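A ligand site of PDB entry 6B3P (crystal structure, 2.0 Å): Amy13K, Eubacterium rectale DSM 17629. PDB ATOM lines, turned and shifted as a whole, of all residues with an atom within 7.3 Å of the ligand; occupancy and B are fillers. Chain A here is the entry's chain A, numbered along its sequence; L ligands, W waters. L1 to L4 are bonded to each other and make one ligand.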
ATOM      1  N   TYR A  18     -19.765 -19.299   9.489  1.00  0.00           N
ATOM      2  CA  TYR A  18     -18.708 -19.447  10.482  1.00  0.00           C
ATOM      3  C   TYR A  18     -18.040 -18.102  10.701  1.00  0.00           C
ATOM      4  O   TYR A  18     -17.566 -17.469   9.754  1.00  0.00           O
ATOM      5  CB  TYR A  18     -17.690 -20.494  10.033  1.00  0.00           C
ATOM      6  CG  TYR A  18     -16.547 -20.689  11.006  1.00  0.00           C
ATOM      7  CD1 TYR A  18     -16.731 -21.331  12.219  1.00  0.00           C
ATOM      8  CD2 TYR A  18     -15.265 -20.231  10.705  1.00  0.00           C
ATOM      9  CE1 TYR A  18     -15.695 -21.509  13.104  1.00  0.00           C
ATOM     10  CE2 TYR A  18     -14.219 -20.408  11.580  1.00  0.00           C
ATOM     11  CZ  TYR A  18     -14.438 -21.049  12.780  1.00  0.00           C
ATOM     12  OH  TYR A  18     -13.393 -21.223  13.664  1.00  0.00           O
ATOM     13  N   ILE A  19     -18.009 -17.666  11.951  1.00  0.00           N
ATOM     14  CA  ILE A  19     -17.502 -16.347  12.310  1.00  0.00           C
ATOM     15  C   ILE A  19     -16.365 -16.520  13.317  1.00  0.00           C
ATOM     16  O   ILE A  19     -16.494 -17.303  14.255  1.00  0.00           O
ATOM     17  CB  ILE A  19     -18.618 -15.460  12.898  1.00  0.00           C
ATOM     18  CG1 ILE A  19     -19.716 -15.239  11.844  1.00  0.00           C
ATOM     19  CG2 ILE A  19     -18.056 -14.112  13.378  1.00  0.00           C
ATOM     20  CD1 ILE A  19     -20.992 -14.662  12.399  1.00  0.00           C
ATOM     21  N   TYR A  20     -15.273 -15.791  13.129  1.00  0.00           N
ATOM     22  CA  TYR A  20     -14.119 -15.960  14.006  1.00  0.00           C
ATOM     23  C   TYR A  20     -13.243 -14.726  14.162  1.00  0.00           C
ATOM     24  O   TYR A  20     -13.129 -13.903  13.251  1.00  0.00           O
ATOM     25  CB  TYR A  20     -13.261 -17.127  13.519  1.00  0.00           C
ATOM     26  CG  TYR A  20     -12.521 -16.872  12.215  1.00  0.00           C
ATOM     27  CD1 TYR A  20     -11.256 -16.302  12.214  1.00  0.00           C
ATOM     28  CD2 TYR A  20     -13.074 -17.225  11.001  1.00  0.00           C
ATOM     29  CE1 TYR A  20     -10.577 -16.076  11.035  1.00  0.00           C
ATOM     30  CE2 TYR A  20     -12.403 -17.006   9.813  1.00  0.00           C
ATOM     31  CZ  TYR A  20     -11.149 -16.430   9.841  1.00  0.00           C
ATOM     32  OH  TYR A  20     -10.453 -16.191   8.669  1.00  0.00           O
ATOM     33  N   LYS A  21     -12.621 -14.628  15.337  1.00  0.00           N
ATOM     34  CA  LYS A  21     -11.619 -13.607  15.633  1.00  0.00           C
ATOM     35  C   LYS A  21     -10.704 -14.086  16.752  1.00  0.00           C
ATOM     36  O   LYS A  21     -11.160 -14.305  17.877  1.00  0.00           O
ATOM     37  CB  LYS A  21     -12.287 -12.278  16.017  1.00  0.00           C
ATOM     38  CG  LYS A  21     -11.304 -11.156  16.349  1.00  0.00           C
ATOM     39  CD  LYS A  21     -10.466 -10.756  15.135  1.00  0.00           C
ATOM     40  CE  LYS A  21      -9.650  -9.501  15.419  1.00  0.00           C
ATOM     41  NZ  LYS A  21      -8.715  -9.139  14.311  1.00  0.00           N
ATOM     42  N   GLU A  22      -9.419 -14.234  16.453  1.00  0.00           N
ATOM     43  CA  GLU A  22      -8.425 -14.683  17.427  1.00  0.00           C
ATOM     44  C   GLU A  22      -8.867 -15.934  18.190  1.00  0.00           C
ATOM     45  O   GLU A  22      -8.764 -15.996  19.416  1.00  0.00           O
ATOM     46  CB  GLU A  22      -8.099 -13.559  18.415  1.00  0.00           C
ATOM     47  CG  GLU A  22      -7.525 -12.299  17.774  1.00  0.00           C
ATOM     48  CD  GLU A  22      -6.166 -12.523  17.134  1.00  0.00           C
ATOM     49  OE1 GLU A  22      -5.548 -13.582  17.394  1.00  0.00           O
ATOM     50  OE2 GLU A  22      -5.703 -11.649  16.384  1.00  0.00           O
ATOM     51  N   THR A  23      -9.368 -16.910  17.436  1.00  0.00           N
ATOM     52  CA  THR A  23      -9.842 -18.200  17.966  1.00  0.00           C
ATOM     53  C   THR A  23     -11.204 -18.122  18.660  1.00  0.00           C
ATOM     54  O   THR A  23     -11.758 -19.153  19.046  1.00  0.00           O
ATOM     55  CB  THR A  23      -8.849 -18.831  18.964  1.00  0.00           C
ATOM     56  OG1 THR A  23      -8.880 -18.116  20.213  1.00  0.00           O
ATOM     57  CG2 THR A  23      -7.428 -18.835  18.406  1.00  0.00           C
ATOM     58  N   ASN A  24     -11.752 -16.918  18.820  1.00  0.00           N
ATOM     59  CA  ASN A  24     -13.131 -16.789  19.280  1.00  0.00           C
ATOM     60  C   ASN A  24     -14.061 -17.213  18.156  1.00  0.00           C
ATOM     61  O   ASN A  24     -13.845 -16.841  17.003  1.00  0.00           O
ATOM     62  CB  ASN A  24     -13.440 -15.361  19.723  1.00  0.00           C
ATOM     63  CG  ASN A  24     -12.575 -14.906  20.886  1.00  0.00           C
ATOM     64  OD1 ASN A  24     -11.901 -13.883  20.831  1.00  0.00           O
ATOM     65  ND2 ASN A  24     -12.604 -15.678  21.964  1.00  0.00           N
ATOM     66  N   LYS A  25     -15.090 -17.996  18.486  1.00  0.00           N
ATOM     67  CA  LYS A  25     -16.019 -18.535  17.490  1.00  0.00           C
ATOM     68  C   LYS A  25     -17.473 -18.322  17.926  1.00  0.00           C
ATOM     69  O   LYS A  25     -18.141 -19.269  18.338  1.00  0.00           O
ATOM     70  CB  LYS A  25     -15.746 -20.025  17.262  1.00  0.00           C
ATOM     71  CG  LYS A  25     -14.299 -20.364  16.936  1.00  0.00           C
ATOM     72  CD  LYS A  25     -14.098 -21.869  16.880  1.00  0.00           C
ATOM     73  CE  LYS A  25     -12.645 -22.239  16.674  1.00  0.00           C
ATOM     74  NZ  LYS A  25     -11.795 -21.938  17.861  1.00  0.00           N
ATOM     75  N   GLU A  29     -18.333 -23.722  16.817  1.00  0.00           N
ATOM     76  CA  GLU A  29     -17.277 -24.437  16.108  1.00  0.00           C
ATOM     77  C   GLU A  29     -17.686 -24.677  14.666  1.00  0.00           C
ATOM     78  O   GLU A  29     -18.872 -24.637  14.337  1.00  0.00           O
ATOM     79  CB  GLU A  29     -16.971 -25.772  16.785  1.00  0.00           C
ATOM     80  CG  GLU A  29     -16.279 -25.661  18.141  1.00  0.00           C
ATOM     81  CD  GLU A  29     -15.882 -27.006  18.709  1.00  0.00           C
ATOM     82  OE1 GLU A  29     -16.095 -28.034  18.023  1.00  0.00           O
ATOM     83  OE2 GLU A  29     -15.370 -27.041  19.842  1.00  0.00           O
ATOM     84  N   TRP A  30     -16.704 -24.908  13.804  1.00  0.00           N
ATOM     85  CA  TRP A  30     -16.954 -25.199  12.391  1.00  0.00           C
ATOM     86  C   TRP A  30     -18.034 -26.273  12.271  1.00  0.00           C
ATOM     87  O   TRP A  30     -18.013 -27.264  13.006  1.00  0.00           O
ATOM     88  CB  TRP A  30     -15.657 -25.662  11.708  1.00  0.00           C
ATOM     89  CG  TRP A  30     -15.827 -25.897  10.247  1.00  0.00           C
ATOM     90  CD1 TRP A  30     -16.036 -27.089   9.622  1.00  0.00           C
ATOM     91  CD2 TRP A  30     -15.809 -24.899   9.212  1.00  0.00           C
ATOM     92  NE1 TRP A  30     -16.153 -26.909   8.265  1.00  0.00           N
ATOM     93  CE2 TRP A  30     -16.017 -25.570   7.986  1.00  0.00           C
ATOM     94  CE3 TRP A  30     -15.648 -23.520   9.208  1.00  0.00           C
ATOM     95  CZ2 TRP A  30     -16.069 -24.895   6.769  1.00  0.00           C
ATOM     96  CZ3 TRP A  30     -15.687 -22.846   8.002  1.00  0.00           C
ATOM     97  CH2 TRP A  30     -15.896 -23.535   6.794  1.00  0.00           C
ATOM     98  N   PRO A  31     -19.000 -26.091  11.335  1.00  0.00           N
ATOM     99  CA  PRO A  31     -19.160 -25.068  10.291  1.00  0.00           C
ATOM    100  C   PRO A  31     -19.863 -23.775  10.718  1.00  0.00           C
ATOM    101  O   PRO A  31     -20.200 -22.971   9.853  1.00  0.00           O
ATOM    102  CB  PRO A  31     -19.993 -25.804   9.246  1.00  0.00           C
ATOM    103  CG  PRO A  31     -20.858 -26.703  10.056  1.00  0.00           C
ATOM    104  CD  PRO A  31     -20.023 -27.141  11.230  1.00  0.00           C
ATOM    105  N   SER A  58     -14.112 -12.186  11.003  1.00  0.00           N
ATOM    106  CA  SER A  58     -14.076 -12.765   9.671  1.00  0.00           C
ATOM    107  C   SER A  58     -15.270 -13.696   9.512  1.00  0.00           C
ATOM    108  O   SER A  58     -15.682 -14.342  10.468  1.00  0.00           O
ATOM    109  CB  SER A  58     -12.779 -13.526   9.431  1.00  0.00           C
ATOM    110  OG  SER A  58     -11.672 -12.651   9.467  1.00  0.00           O
ATOM    111  N   ILE A  60     -16.918 -16.868   7.118  1.00  0.00           N
ATOM    112  CA  ILE A  60     -16.820 -17.890   6.084  1.00  0.00           C
ATOM    113  C   ILE A  60     -18.185 -18.533   5.882  1.00  0.00           C
ATOM    114  O   ILE A  60     -18.696 -19.224   6.764  1.00  0.00           O
ATOM    115  CB  ILE A  60     -15.777 -18.983   6.435  1.00  0.00           C
ATOM    116  CG1 ILE A  60     -14.380 -18.379   6.471  1.00  0.00           C
ATOM    117  CG2 ILE A  60     -15.833 -20.126   5.416  1.00  0.00           C
ATOM    118  CD1 ILE A  60     -13.311 -19.323   6.981  1.00  0.00           C
ATOM    119  N   ASN A  62     -20.446 -21.323   4.112  1.00  0.00           N
ATOM    120  CA  ASN A  62     -20.135 -22.705   3.781  1.00  0.00           C
ATOM    121  C   ASN A  62     -21.415 -23.540   3.646  1.00  0.00           C
ATOM    122  O   ASN A  62     -22.498 -23.058   3.959  1.00  0.00           O
ATOM    123  CB  ASN A  62     -19.214 -23.308   4.850  1.00  0.00           C
ATOM    124  CG  ASN A  62     -19.854 -23.330   6.223  1.00  0.00           C
ATOM    125  OD1 ASN A  62     -20.811 -24.054   6.460  1.00  0.00           O
ATOM    126  ND2 ASN A  62     -19.301 -22.546   7.148  1.00  0.00           N
ATOM    127  N   GLY A  65     -20.765 -27.972   6.644  1.00  0.00           N
ATOM    128  CA  GLY A  65     -19.943 -29.115   7.001  1.00  0.00           C
ATOM    129  C   GLY A  65     -19.843 -30.197   5.936  1.00  0.00           C
ATOM    130  O   GLY A  65     -19.462 -31.325   6.263  1.00  0.00           O
ATOM    131  N   GLY A  67     -18.066 -29.933   2.903  1.00  0.00           N
ATOM    132  CA  GLY A  67     -16.875 -29.913   2.076  1.00  0.00           C
ATOM    133  C   GLY A  67     -16.626 -28.669   1.241  1.00  0.00           C
ATOM    134  O   GLY A  67     -15.587 -28.593   0.566  1.00  0.00           O
ATOM    135  N   GLN A  69     -16.740 -24.241   0.958  1.00  0.00           N
ATOM    136  CA  GLN A  69     -16.806 -22.946   1.624  1.00  0.00           C
ATOM    137  C   GLN A  69     -16.306 -21.836   0.703  1.00  0.00           C
ATOM    138  O   GLN A  69     -15.459 -22.063  -0.157  1.00  0.00           O
ATOM    139  CB  GLN A  69     -15.981 -22.953   2.904  1.00  0.00           C
ATOM    140  CG  GLN A  69     -14.496 -23.021   2.640  1.00  0.00           C
ATOM    141  CD  GLN A  69     -13.691 -23.331   3.872  1.00  0.00           C
ATOM    142  OE1 GLN A  69     -13.805 -24.400   4.468  1.00  0.00           O
ATOM    143  NE2 GLN A  69     -12.861 -22.366   4.275  1.00  0.00           N
ATOM    144  N   LEU A  70     -16.843 -20.643   0.911  1.00  0.00           N
ATOM    145  CA  LEU A  70     -16.385 -19.463   0.186  1.00  0.00           C
ATOM    146  C   LEU A  70     -15.184 -18.841   0.899  1.00  0.00           C
ATOM    147  O   LEU A  70     -14.908 -19.151   2.057  1.00  0.00           O
ATOM    148  CB  LEU A  70     -17.512 -18.449   0.041  1.00  0.00           C
ATOM    149  CG  LEU A  70     -18.824 -18.990  -0.537  1.00  0.00           C
ATOM    150  CD1 LEU A  70     -19.828 -17.860  -0.697  1.00  0.00           C
ATOM    151  CD2 LEU A  70     -18.596 -19.695  -1.864  1.00  0.00           C
ATOM    152  N   ASP A  72     -12.860 -16.183   2.882  1.00  0.00           N
ATOM    153  CA  ASP A  72     -13.123 -15.324   4.043  1.00  0.00           C
ATOM    154  C   ASP A  72     -13.413 -13.883   3.637  1.00  0.00           C
ATOM    155  O   ASP A  72     -12.776 -13.354   2.728  1.00  0.00           O
ATOM    156  CB  ASP A  72     -11.934 -15.334   5.002  1.00  0.00           C
ATOM    157  CG  ASP A  72     -11.432 -16.728   5.317  1.00  0.00           C
ATOM    158  OD1 ASP A  72     -11.449 -17.588   4.419  1.00  0.00           O
ATOM    159  OD2 ASP A  72     -11.021 -16.948   6.471  1.00  0.00           O
HETATM  160  C1  LIG L   1      -9.962 -30.626   8.396  1.00  0.00           C
HETATM  161  C2  LIG L   1     -11.211 -30.247   7.627  1.00  0.00           C
HETATM  162  C3  LIG L   1     -11.474 -28.748   7.596  1.00  0.00           C
HETATM  163  C4  LIG L   1     -11.250 -28.081   8.942  1.00  0.00           C
HETATM  164  C5  LIG L   1      -9.934 -28.555   9.537  1.00  0.00           C
HETATM  165  C6  LIG L   1      -9.768 -28.059  10.943  1.00  0.00           C
HETATM  166  O1  LIG L   1      -8.827 -30.306   7.614  1.00  0.00           O
HETATM  167  O2  LIG L   1     -11.070 -30.673   6.276  1.00  0.00           O
HETATM  168  O3  LIG L   1     -12.808 -28.585   7.138  1.00  0.00           O
HETATM  169  O4  LIG L   1     -11.175 -26.676   8.784  1.00  0.00           O
HETATM  170  O5  LIG L   1      -9.866 -29.955   9.615  1.00  0.00           O
HETATM  171  O6  LIG L   1      -8.618 -27.227  10.998  1.00  0.00           O
HETATM  172  C1  LG2 L   2     -12.389 -25.981   8.904  1.00  0.00           C
HETATM  173  C2  LG2 L   2     -12.512 -24.992   7.757  1.00  0.00           C
HETATM  174  C3  LG2 L   2     -11.466 -23.902   7.934  1.00  0.00           C
HETATM  175  C4  LG2 L   2     -11.563 -23.277   9.309  1.00  0.00           C
HETATM  176  C5  LG2 L   2     -11.539 -24.335  10.379  1.00  0.00           C
HETATM  177  C6  LG2 L   2     -11.716 -23.681  11.750  1.00  0.00           C
HETATM  178  O1  LG2 L   2     -12.392 -25.657   6.516  1.00  0.00           O
HETATM  179  O2  LG2 L   2     -11.613 -22.912   6.967  1.00  0.00           O
HETATM  180  O3  LG2 L   2     -10.509 -22.347   9.492  1.00  0.00           O
HETATM  181  O4  LG2 L   2     -12.548 -25.260  10.122  1.00  0.00           O
HETATM  182  O5  LG2 L   2     -11.874 -24.591  12.797  1.00  0.00           O
HETATM  183  C1  LG3 L   3     -10.883 -20.973   9.438  1.00  0.00           C
HETATM  184  C2  LG3 L   3      -9.928 -20.217   8.547  1.00  0.00           C
HETATM  185  C3  LG3 L   3      -8.587 -20.004   9.218  1.00  0.00           C
HETATM  186  C4  LG3 L   3      -8.775 -19.442  10.612  1.00  0.00           C
HETATM  187  C5  LG3 L   3      -9.790 -20.262  11.394  1.00  0.00           C
HETATM  188  C6  LG3 L   3     -10.086 -19.729  12.793  1.00  0.00           C
HETATM  189  O1  LG3 L   3      -9.816 -20.926   7.354  1.00  0.00           O
HETATM  190  O2  LG3 L   3      -7.777 -19.172   8.430  1.00  0.00           O
HETATM  191  O3  LG3 L   3      -7.517 -19.420  11.242  1.00  0.00           O
HETATM  192  O4  LG3 L   3     -10.980 -20.315  10.662  1.00  0.00           O
HETATM  193  O5  LG3 L   3     -10.978 -20.517  13.528  1.00  0.00           O
HETATM  194  C1  LG4 L   4      -6.869 -18.153  11.265  1.00  0.00           C
HETATM  195  C2  LG4 L   4      -5.398 -18.314  10.993  1.00  0.00           C
HETATM  196  C3  LG4 L   4      -4.686 -18.934  12.196  1.00  0.00           C
HETATM  197  C4  LG4 L   4      -4.977 -18.155  13.460  1.00  0.00           C
HETATM  198  C5  LG4 L   4      -6.482 -18.002  13.605  1.00  0.00           C
HETATM  199  C6  LG4 L   4      -6.865 -17.119  14.771  1.00  0.00           C
HETATM  200  O1  LG4 L   4      -5.181 -19.093   9.853  1.00  0.00           O
HETATM  201  O2  LG4 L   4      -3.317 -18.969  11.924  1.00  0.00           O
HETATM  202  O3  LG4 L   4      -4.334 -18.738  14.602  1.00  0.00           O
HETATM  203  O4  LG4 L   4      -7.027 -17.418  12.457  1.00  0.00           O
HETATM  204  O5  LG4 L   4      -8.223 -16.760  14.708  1.00  0.00           O
HETATM  205  O   HOH W   1     -10.198 -25.502   4.938  1.00  0.00           O
HETATM  206  O   HOH W   2      -9.424 -19.246   5.176  1.00  0.00           O
HETATM  207  O   HOH W   3      -9.284 -24.233  14.031  1.00  0.00           O
HETATM  208  O   HOH W   4     -14.637 -30.089   8.697  1.00  0.00           O
HETATM  209  O   HOH W   5     -13.907 -24.720  14.621  1.00  0.00           O
HETATM  210  O   HOH W   6      -5.436 -14.831  11.346  1.00  0.00           O
HETATM  211  O   HOH W   7     -12.729 -27.620  12.566  1.00  0.00           O
HETATM  212  O   HOH W   8      -2.272 -16.302  11.489  1.00  0.00           O
HETATM  213  O   HOH W   9      -5.143 -21.941  10.129  1.00  0.00           O
HETATM  214  O   HOH W  10     -13.336 -32.829   7.294  1.00  0.00           O
HETATM  215  O   HOH W  11      -2.316 -21.458  12.292  1.00  0.00           O
HETATM  216  O   HOH W  12      -7.994 -17.207   6.720  1.00  0.00           O
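Water W12 lies within hydrogen-bond range of O2 of LG3 L3 (2.6 Å), OD2 of Asp 72 (3.0 Å) and OH of Tyr 20 (3.3 Å). Water W5 bridges O5 of LG2 L2 and N of Trp 30. Water W2 bridges OD1 of Asp 72 and O1 of LG3 L3.
Residues that only touch the ligand: Tyr 20 (3.7 Å), Lys 25 (3.95 Å), Trp 30 (3.3 Å) and Ile 60 (3.8 Å). Hydrophobic or aromatic side chains within 4 Å of the ligand: Tyr 18, Tyr 20, Trp 30 and Ile 60. Along chain A the residues within 4 Å of the ligand span positions 18 to 69. The nearest printed residue that does not touch the ligand is Asp 72 (4.02 Å).
The backbone carbonyl oxygen (O) of Tyr 18 sits at hydrogen-bond distance from the backbone NH (N) of Ile 60. NZ of Lys 25 is in hydrogen-bond range of O of Thr 23, at 3.0 Å. The backbone carbonyl oxygen of Tyr 20 sits at hydrogen-bond distance from the backbone NH of Ser 58, 3.0 Å away. O of Ile 60 is in hydrogen-bond range of ND2 of Asn 62 (3.4 Å).
An oxygen (O5) of LG3 L3 sits at hydrogen-bond distance from the side-chain hydroxyl (OH) of Tyr 18 (2.5 Å). OE1 of Gln 69 sits at hydrogen-bond distance from O1 of LG2 L2 (2.8 Å). The backbone NH (N) of Thr 23 is in hydrogen-bond range of an oxygen (O5) of LG4 L4. The backbone NH (N) of Glu 22 lies within hydrogen-bond range of an oxygen (O5) of LG4 L4 (3.3 Å).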
